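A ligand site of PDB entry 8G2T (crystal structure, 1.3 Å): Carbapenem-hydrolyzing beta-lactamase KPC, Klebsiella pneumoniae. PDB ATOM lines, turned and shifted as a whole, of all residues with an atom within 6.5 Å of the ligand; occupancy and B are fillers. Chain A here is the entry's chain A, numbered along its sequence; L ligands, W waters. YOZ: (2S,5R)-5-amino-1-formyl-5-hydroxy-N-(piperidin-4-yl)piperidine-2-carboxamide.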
ATOM      1  N   LEU A  44       5.519  16.265 -14.491  1.00  0.00           N
ATOM      2  CA  LEU A  44       5.929  17.665 -14.763  1.00  0.00           C
ATOM      3  C   LEU A  44       4.693  18.540 -14.996  1.00  0.00           C
ATOM      4  O   LEU A  44       4.694  19.706 -14.580  1.00  0.00           O
ATOM      5  CB  LEU A  44       6.835  17.715 -15.980  1.00  0.00           C
ATOM      6  CG  LEU A  44       8.253  17.223 -15.723  1.00  0.00           C
ATOM      7  CD1 LEU A  44       8.978  16.910 -17.019  1.00  0.00           C
ATOM      8  CD2 LEU A  44       9.036  18.244 -14.898  1.00  0.00           C
ATOM      9  N   CYS A  45       3.701  18.040 -15.734  1.00  0.00           N
ATOM     10  CA  CYS A  45       2.568  18.883 -16.168  1.00  0.00           C
ATOM     11  C   CYS A  45       3.153  20.144 -16.846  1.00  0.00           C
ATOM     12  O   CYS A  45       4.189  20.021 -17.533  1.00  0.00           O
ATOM     13  CB  CYS A  45       1.650  19.192 -14.992  1.00  0.00           C
ATOM     14  SG  CYS A  45       1.298  17.729 -13.970  1.00  0.00           S
ATOM     15  N   SER A  46       2.544  21.315 -16.698  1.00  0.00           N
ATOM     16  CA  SER A  46       2.987  22.530 -17.431  1.00  0.00           C
ATOM     17  C   SER A  46       4.362  22.994 -16.951  1.00  0.00           C
ATOM     18  O   SER A  46       4.909  23.914 -17.569  1.00  0.00           O
ATOM     19  CB  SER A  46       2.059  23.690 -17.285  1.00  0.00           C
ATOM     20  OG  SER A  46       0.847  23.457 -18.012  1.00  0.00           O
ATOM     21  N   SER A  47       4.899  22.422 -15.871  1.00  0.00           N
ATOM     22  CA  SER A  47       6.147  22.957 -15.284  1.00  0.00           C
ATOM     23  C   SER A  47       7.313  22.748 -16.248  1.00  0.00           C
ATOM     24  O   SER A  47       8.333  23.425 -16.100  1.00  0.00           O
ATOM     25  CB  SER A  47       6.432  22.425 -13.895  1.00  0.00           C
ATOM     26  OG  SER A  47       6.941  21.107 -13.913  1.00  0.00           O
ATOM     27  N   LYS A  49       7.521  23.940 -19.029  1.00  0.00           N
ATOM     28  CA  LYS A  49       7.614  25.157 -19.875  1.00  0.00           C
ATOM     29  C   LYS A  49       8.729  26.090 -19.388  1.00  0.00           C
ATOM     30  O   LYS A  49       9.271  26.824 -20.205  1.00  0.00           O
ATOM     31  CB  LYS A  49       6.258  25.856 -19.911  1.00  0.00           C
ATOM     32  CG  LYS A  49       5.200  25.094 -20.692  1.00  0.00           C
ATOM     33  CD  LYS A  49       3.800  25.596 -20.473  1.00  0.00           C
ATOM     34  CE  LYS A  49       2.779  24.813 -21.272  1.00  0.00           C
ATOM     35  NZ  LYS A  49       1.409  24.908 -20.707  1.00  0.00           N
ATOM     36  N   PRO A  80      -6.236  24.533 -26.876  1.00  0.00           N
ATOM     37  CA  PRO A  80      -6.932  25.134 -25.738  1.00  0.00           C
ATOM     38  C   PRO A  80      -5.956  25.836 -24.767  1.00  0.00           C
ATOM     39  O   PRO A  80      -4.803  25.382 -24.592  1.00  0.00           O
ATOM     40  CB  PRO A  80      -7.596  23.930 -25.096  1.00  0.00           C
ATOM     41  CG  PRO A  80      -7.920  23.060 -26.297  1.00  0.00           C
ATOM     42  CD  PRO A  80      -6.672  23.148 -27.156  1.00  0.00           C
ATOM     43  N   TRP A  81      -6.428  26.927 -24.188  1.00  0.00           N
ATOM     44  CA  TRP A  81      -5.635  27.761 -23.235  1.00  0.00           C
ATOM     45  C   TRP A  81      -4.351  28.248 -23.921  1.00  0.00           C
ATOM     46  O   TRP A  81      -3.228  28.019 -23.395  1.00  0.00           O
ATOM     47  CB  TRP A  81      -5.359  27.026 -21.925  1.00  0.00           C
ATOM     48  CG  TRP A  81      -6.614  26.488 -21.302  1.00  0.00           C
ATOM     49  CD1 TRP A  81      -7.653  27.185 -20.768  1.00  0.00           C
ATOM     50  CD2 TRP A  81      -6.926  25.103 -21.147  1.00  0.00           C
ATOM     51  NE1 TRP A  81      -8.598  26.319 -20.286  1.00  0.00           N
ATOM     52  CE2 TRP A  81      -8.169  25.036 -20.488  1.00  0.00           C
ATOM     53  CE3 TRP A  81      -6.257  23.915 -21.455  1.00  0.00           C
ATOM     54  CZ2 TRP A  81      -8.793  23.822 -20.202  1.00  0.00           C
ATOM     55  CZ3 TRP A  81      -6.860  22.714 -21.165  1.00  0.00           C
ATOM     56  CH2 TRP A  81      -8.099  22.675 -20.520  1.00  0.00           C
ATOM     57  N   SER A  82      -4.518  28.993 -24.986  1.00  0.00           N
ATOM     58  CA  SER A  82      -3.451  29.725 -25.720  1.00  0.00           C
ATOM     59  C   SER A  82      -3.895  31.176 -25.836  1.00  0.00           C
ATOM     60  O   SER A  82      -3.990  31.717 -26.932  1.00  0.00           O
ATOM     61  CB  SER A  82      -3.163  29.085 -27.046  1.00  0.00           C
ATOM     62  OG  SER A  82      -2.801  27.732 -26.868  1.00  0.00           O
ATOM     63  N   TYR A 105       1.971  32.563 -18.648  1.00  0.00           N
ATOM     64  CA  TYR A 105       0.526  32.260 -18.818  1.00  0.00           C
ATOM     65  C   TYR A 105       0.312  30.782 -19.105  1.00  0.00           C
ATOM     66  O   TYR A 105      -0.835  30.378 -19.211  1.00  0.00           O
ATOM     67  CB  TYR A 105      -0.059  33.129 -19.924  1.00  0.00           C
ATOM     68  CG  TYR A 105      -0.113  34.581 -19.538  1.00  0.00           C
ATOM     69  CD1 TYR A 105       0.958  35.427 -19.783  1.00  0.00           C
ATOM     70  CD2 TYR A 105      -1.188  35.093 -18.839  1.00  0.00           C
ATOM     71  CE1 TYR A 105       0.937  36.749 -19.393  1.00  0.00           C
ATOM     72  CE2 TYR A 105      -1.215  36.419 -18.428  1.00  0.00           C
ATOM     73  CZ  TYR A 105      -0.161  37.254 -18.713  1.00  0.00           C
ATOM     74  OH  TYR A 105      -0.150  38.553 -18.306  1.00  0.00           O
ATOM     75  N   SER A 106       1.373  29.986 -19.242  1.00  0.00           N
ATOM     76  CA  SER A 106       1.271  28.547 -19.593  1.00  0.00           C
ATOM     77  C   SER A 106       0.617  28.397 -20.975  1.00  0.00           C
ATOM     78  O   SER A 106      -0.017  27.381 -21.209  1.00  0.00           O
ATOM     79  CB  SER A 106       0.498  27.799 -18.537  1.00  0.00           C
ATOM     80  OG  SER A 106       1.070  26.527 -18.315  1.00  0.00           O
ATOM     81  N   ASP A 107       0.807  29.371 -21.854  1.00  0.00           N
ATOM     82  CA  ASP A 107       0.193  29.365 -23.204  1.00  0.00           C
ATOM     83  C   ASP A 107       0.642  28.087 -23.930  1.00  0.00           C
ATOM     84  O   ASP A 107       1.851  27.903 -24.156  1.00  0.00           O
ATOM     85  CB  ASP A 107       0.588  30.634 -23.947  1.00  0.00           C
ATOM     86  CG  ASP A 107      -0.139  30.807 -25.271  1.00  0.00           C
ATOM     87  OD1 ASP A 107       0.109  29.984 -26.179  1.00  0.00           O
ATOM     88  OD2 ASP A 107      -0.939  31.762 -25.377  1.00  0.00           O
ATOM     89  N   ASN A 108      -0.309  27.232 -24.319  1.00  0.00           N
ATOM     90  CA  ASN A 108       0.036  25.900 -24.862  1.00  0.00           C
ATOM     91  C   ASN A 108       0.560  26.001 -26.294  1.00  0.00           C
ATOM     92  O   ASN A 108       1.508  25.274 -26.636  1.00  0.00           O
ATOM     93  CB  ASN A 108      -1.130  24.922 -24.713  1.00  0.00           C
ATOM     94  CG  ASN A 108      -1.393  24.615 -23.265  1.00  0.00           C
ATOM     95  OD1 ASN A 108      -0.468  24.211 -22.545  1.00  0.00           O
ATOM     96  ND2 ASN A 108      -2.590  24.887 -22.768  1.00  0.00           N
ATOM     97  N   GLU A 142       1.911  19.614 -25.619  1.00  0.00           N
ATOM     98  CA  GLU A 142       0.604  19.933 -24.997  1.00  0.00           C
ATOM     99  C   GLU A 142      -0.488  19.561 -26.004  1.00  0.00           C
ATOM    100  O   GLU A 142      -0.316  19.821 -27.192  1.00  0.00           O
ATOM    101  CB  GLU A 142       0.550  21.410 -24.588  1.00  0.00           C
ATOM    102  CG  GLU A 142       1.418  21.738 -23.386  1.00  0.00           C
ATOM    103  CD  GLU A 142       0.859  21.318 -22.042  1.00  0.00           C
ATOM    104  OE1 GLU A 142      -0.117  20.518 -22.015  1.00  0.00           O
ATOM    105  OE2 GLU A 142       1.388  21.805 -21.001  1.00  0.00           O
ATOM    106  N   LEU A 143      -1.616  18.964 -25.571  1.00  0.00           N
ATOM    107  CA  LEU A 143      -2.044  18.685 -24.206  1.00  0.00           C
ATOM    108  C   LEU A 143      -1.931  17.177 -23.909  1.00  0.00           C
ATOM    109  O   LEU A 143      -2.873  16.636 -23.302  1.00  0.00           O
ATOM    110  CB  LEU A 143      -3.517  19.073 -24.054  1.00  0.00           C
ATOM    111  CG  LEU A 143      -3.881  20.530 -24.327  1.00  0.00           C
ATOM    112  CD1 LEU A 143      -5.365  20.668 -24.626  1.00  0.00           C
ATOM    113  CD2 LEU A 143      -3.480  21.392 -23.150  1.00  0.00           C
ATOM    114  N   ASN A 146      -0.187  14.999 -19.859  1.00  0.00           N
ATOM    115  CA  ASN A 146      -0.819  15.391 -18.571  1.00  0.00           C
ATOM    116  C   ASN A 146      -1.631  14.253 -17.936  1.00  0.00           C
ATOM    117  O   ASN A 146      -2.363  14.538 -16.967  1.00  0.00           O
ATOM    118  CB  ASN A 146      -1.693  16.626 -18.777  1.00  0.00           C
ATOM    119  CG  ASN A 146      -0.891  17.753 -19.365  1.00  0.00           C
ATOM    120  OD1 ASN A 146       0.229  18.014 -18.901  1.00  0.00           O
ATOM    121  ND2 ASN A 146      -1.424  18.397 -20.396  1.00  0.00           N
ATOM    122  N   THR A 192       0.679  32.604 -12.708  1.00  0.00           N
ATOM    123  CA  THR A 192      -0.156  31.426 -12.346  1.00  0.00           C
ATOM    124  C   THR A 192       0.182  30.858 -10.959  1.00  0.00           C
ATOM    125  O   THR A 192      -0.468  29.881 -10.563  1.00  0.00           O
ATOM    126  CB  THR A 192      -0.016  30.326 -13.398  1.00  0.00           C
ATOM    127  OG1 THR A 192       1.326  29.827 -13.332  1.00  0.00           O
ATOM    128  CG2 THR A 192      -0.348  30.810 -14.796  1.00  0.00           C
ATOM    129  N   LYS A 210       7.585  28.677 -11.810  1.00  0.00           N
ATOM    130  CA  LYS A 210       6.690  28.078 -12.815  1.00  0.00           C
ATOM    131  C   LYS A 210       5.906  26.971 -12.145  1.00  0.00           C
ATOM    132  O   LYS A 210       6.488  26.080 -11.527  1.00  0.00           O
ATOM    133  CB  LYS A 210       7.470  27.524 -14.018  1.00  0.00           C
ATOM    134  CG  LYS A 210       6.559  26.903 -15.075  1.00  0.00           C
ATOM    135  CD  LYS A 210       5.701  27.894 -15.860  1.00  0.00           C
ATOM    136  CE  LYS A 210       4.615  27.262 -16.695  1.00  0.00           C
ATOM    137  NZ  LYS A 210       3.377  27.077 -15.910  1.00  0.00           N
ATOM    138  N   THR A 211       4.594  26.985 -12.383  1.00  0.00           N
ATOM    139  CA  THR A 211       3.642  25.985 -11.850  1.00  0.00           C
ATOM    140  C   THR A 211       3.401  24.872 -12.880  1.00  0.00           C
ATOM    141  O   THR A 211       3.692  25.036 -14.097  1.00  0.00           O
ATOM    142  CB  THR A 211       2.299  26.647 -11.532  1.00  0.00           C
ATOM    143  OG1 THR A 211       1.762  27.191 -12.744  1.00  0.00           O
ATOM    144  CG2 THR A 211       2.400  27.748 -10.492  1.00  0.00           C
ATOM    145  N   GLY A 212       2.859  23.770 -12.397  1.00  0.00           N
ATOM    146  CA  GLY A 212       2.259  22.748 -13.261  1.00  0.00           C
ATOM    147  C   GLY A 212       1.046  22.184 -12.584  1.00  0.00           C
ATOM    148  O   GLY A 212       1.014  22.070 -11.356  1.00  0.00           O
ATOM    149  N   THR A 213       0.023  21.858 -13.359  1.00  0.00           N
ATOM    150  CA  THR A 213      -1.245  21.347 -12.791  1.00  0.00           C
ATOM    151  C   THR A 213      -1.837  20.316 -13.755  1.00  0.00           C
ATOM    152  O   THR A 213      -2.451  20.722 -14.709  1.00  0.00           O
ATOM    153  CB  THR A 213      -2.222  22.504 -12.540  1.00  0.00           C
ATOM    154  OG1 THR A 213      -1.527  23.601 -11.951  1.00  0.00           O
ATOM    155  CG2 THR A 213      -3.361  22.075 -11.650  1.00  0.00           C
ATOM    156  N   CYS A 214      -1.688  19.031 -13.493  1.00  0.00           N
ATOM    157  CA  CYS A 214      -2.364  17.968 -14.272  1.00  0.00           C
ATOM    158  C   CYS A 214      -3.774  17.781 -13.710  1.00  0.00           C
ATOM    159  O   CYS A 214      -4.658  17.406 -14.488  1.00  0.00           O
ATOM    160  CB  CYS A 214      -1.615  16.637 -14.220  1.00  0.00           C
ATOM    161  SG  CYS A 214      -0.063  16.618 -15.145  1.00  0.00           S
ATOM    162  N   GLY A 215      -3.997  18.029 -12.426  1.00  0.00           N
ATOM    163  CA  GLY A 215      -5.319  17.973 -11.773  1.00  0.00           C
ATOM    164  C   GLY A 215      -5.714  16.547 -11.431  1.00  0.00           C
ATOM    165  O   GLY A 215      -6.007  16.272 -10.255  1.00  0.00           O
HETATM  166  N1  YOZ L   1      -4.339  20.919 -17.028  1.00  0.00           N
HETATM  167  C1  YOZ L   1      -3.162  21.392 -17.727  1.00  0.00           C
HETATM  168  O1  YOZ L   1      -2.170  20.366 -17.710  1.00  0.00           O
HETATM  169  C2  YOZ L   1      -3.481  21.764 -19.181  1.00  0.00           C
HETATM  170  C3  YOZ L   1      -2.283  22.416 -19.869  1.00  0.00           C
HETATM  171  C4  YOZ L   1      -1.713  23.577 -19.063  1.00  0.00           C
HETATM  172  C5  YOZ L   1      -2.605  24.807 -19.136  1.00  0.00           C
HETATM  173  O2  YOZ L   1      -3.266  25.041 -20.152  1.00  0.00           O
HETATM  174  N2  YOZ L   1      -2.679  25.626 -18.085  1.00  0.00           N
HETATM  175  C6  YOZ L   1      -3.454  26.859 -18.107  1.00  0.00           C
HETATM  176  C7  YOZ L   1      -3.063  27.802 -16.976  1.00  0.00           C
HETATM  177  C8  YOZ L   1      -3.885  29.080 -17.005  1.00  0.00           C
HETATM  178  N3  YOZ L   1      -5.314  28.773 -16.959  1.00  0.00           N
HETATM  179  C9  YOZ L   1      -5.736  27.842 -18.011  1.00  0.00           C
HETATM  180  C10 YOZ L   1      -4.935  26.549 -17.999  1.00  0.00           C
HETATM  181  N4  YOZ L   1      -1.456  23.122 -17.682  1.00  0.00           N
HETATM  182  C11 YOZ L   1      -0.258  23.093 -17.072  1.00  0.00           C
HETATM  183  O3  YOZ L   1       0.015  22.483 -16.049  1.00  0.00           O
HETATM  184  C12 YOZ L   1      -2.632  22.626 -16.992  1.00  0.00           C
HETATM  185  O   HOH W   1      -4.991  30.252 -20.184  1.00  0.00           O
HETATM  186  O   HOH W   2      -5.425  18.749 -18.192  1.00  0.00           O
HETATM  187  O   HOH W   3       0.497  20.476 -18.793  1.00  0.00           O
HETATM  188  O   HOH W   4      -3.076  28.024 -13.568  1.00  0.00           O
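OG of Ser 46 is bonded to C11 of the ligand (1.5 Å). The backbone carbonyl oxygen (O) of Thr 213 lies close to a nitrogen (N1) of the ligand. N of Ser 46 lies close to O3 of the ligand. N of Thr 213 lies within hydrogen-bond range of O3 of the ligand (2.8 Å). The side-chain amide nitrogen (ND2) of Asn 108 is in hydrogen-bond range of an oxygen (O2) of the ligand, 2.7 Å away. The side-chain amide nitrogen of Asn 146 lies close to an oxygen (O1) of the ligand (3.4 Å).
Residues that only touch the ligand: Cys 45 (3.8 Å), Lys 49 (3.8 Å), Trp 81 (3.4 Å), Tyr 105 (3.98 Å), Ser 106 (3.9 Å), Glu 142 (3.6 Å), Leu 143 (3.6 Å) and Gly 212 (3.6 Å). Hydrophobic or aromatic side chains within 4 Å of the ligand: Trp 81 and Leu 143. 12 residues have an atom within 4 Å of the ligand: Cys 45, Ser 46, Lys 49, Trp 81, Tyr 105, Ser 106, Asn 108, Glu 142, Leu 143, Asn 146, Gly 212 and Thr 213. Along chain A the residues within 4 Å of the ligand span positions 45 to 213. The nearest printed residue that does not touch the ligand is Cys 214 (4.2 Å).
Water W3 lies within hydrogen-bond range of the side-chain amide oxygen of Asn 146 (2.5 Å), the side-chain carboxylate of Glu 142 (2.7 Å), an oxygen (O1) of the ligand (2.9 Å) and the backbone NH of Ser 46 (3.0 Å).
The side-chain amide oxygen (OD1) of Asn 108 lies close to the backbone carbonyl oxygen (O) of Ser 106 (3.5 Å). The backbone carbonyl oxygen of Trp 81 lies within hydrogen-bond range of the backbone NH of Asn 108 (3.2 Å). ND2 of Asn 146 sits at hydrogen-bond distance from OE1 of Glu 142, at 3.0 Å. OD1 of Asn 108 is in hydrogen-bond range of NZ of Lys 49 (2.7 Å). O of Pro 80 sits at hydrogen-bond distance from ND2 of Asn 108 (2.9 Å). The backbone carbonyl oxygen of Ser 106 is in hydrogen-bond range of the side-chain amino group of Lys 49 (2.9 Å). OG of Ser 106 is in hydrogen-bond range of OG of Ser 46, at 3.1 Å. The side-chain amide oxygen (OD1) of Asn 108 lies close to the side-chain carboxylate (OE2) of Glu 142, 3.4 Å away.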
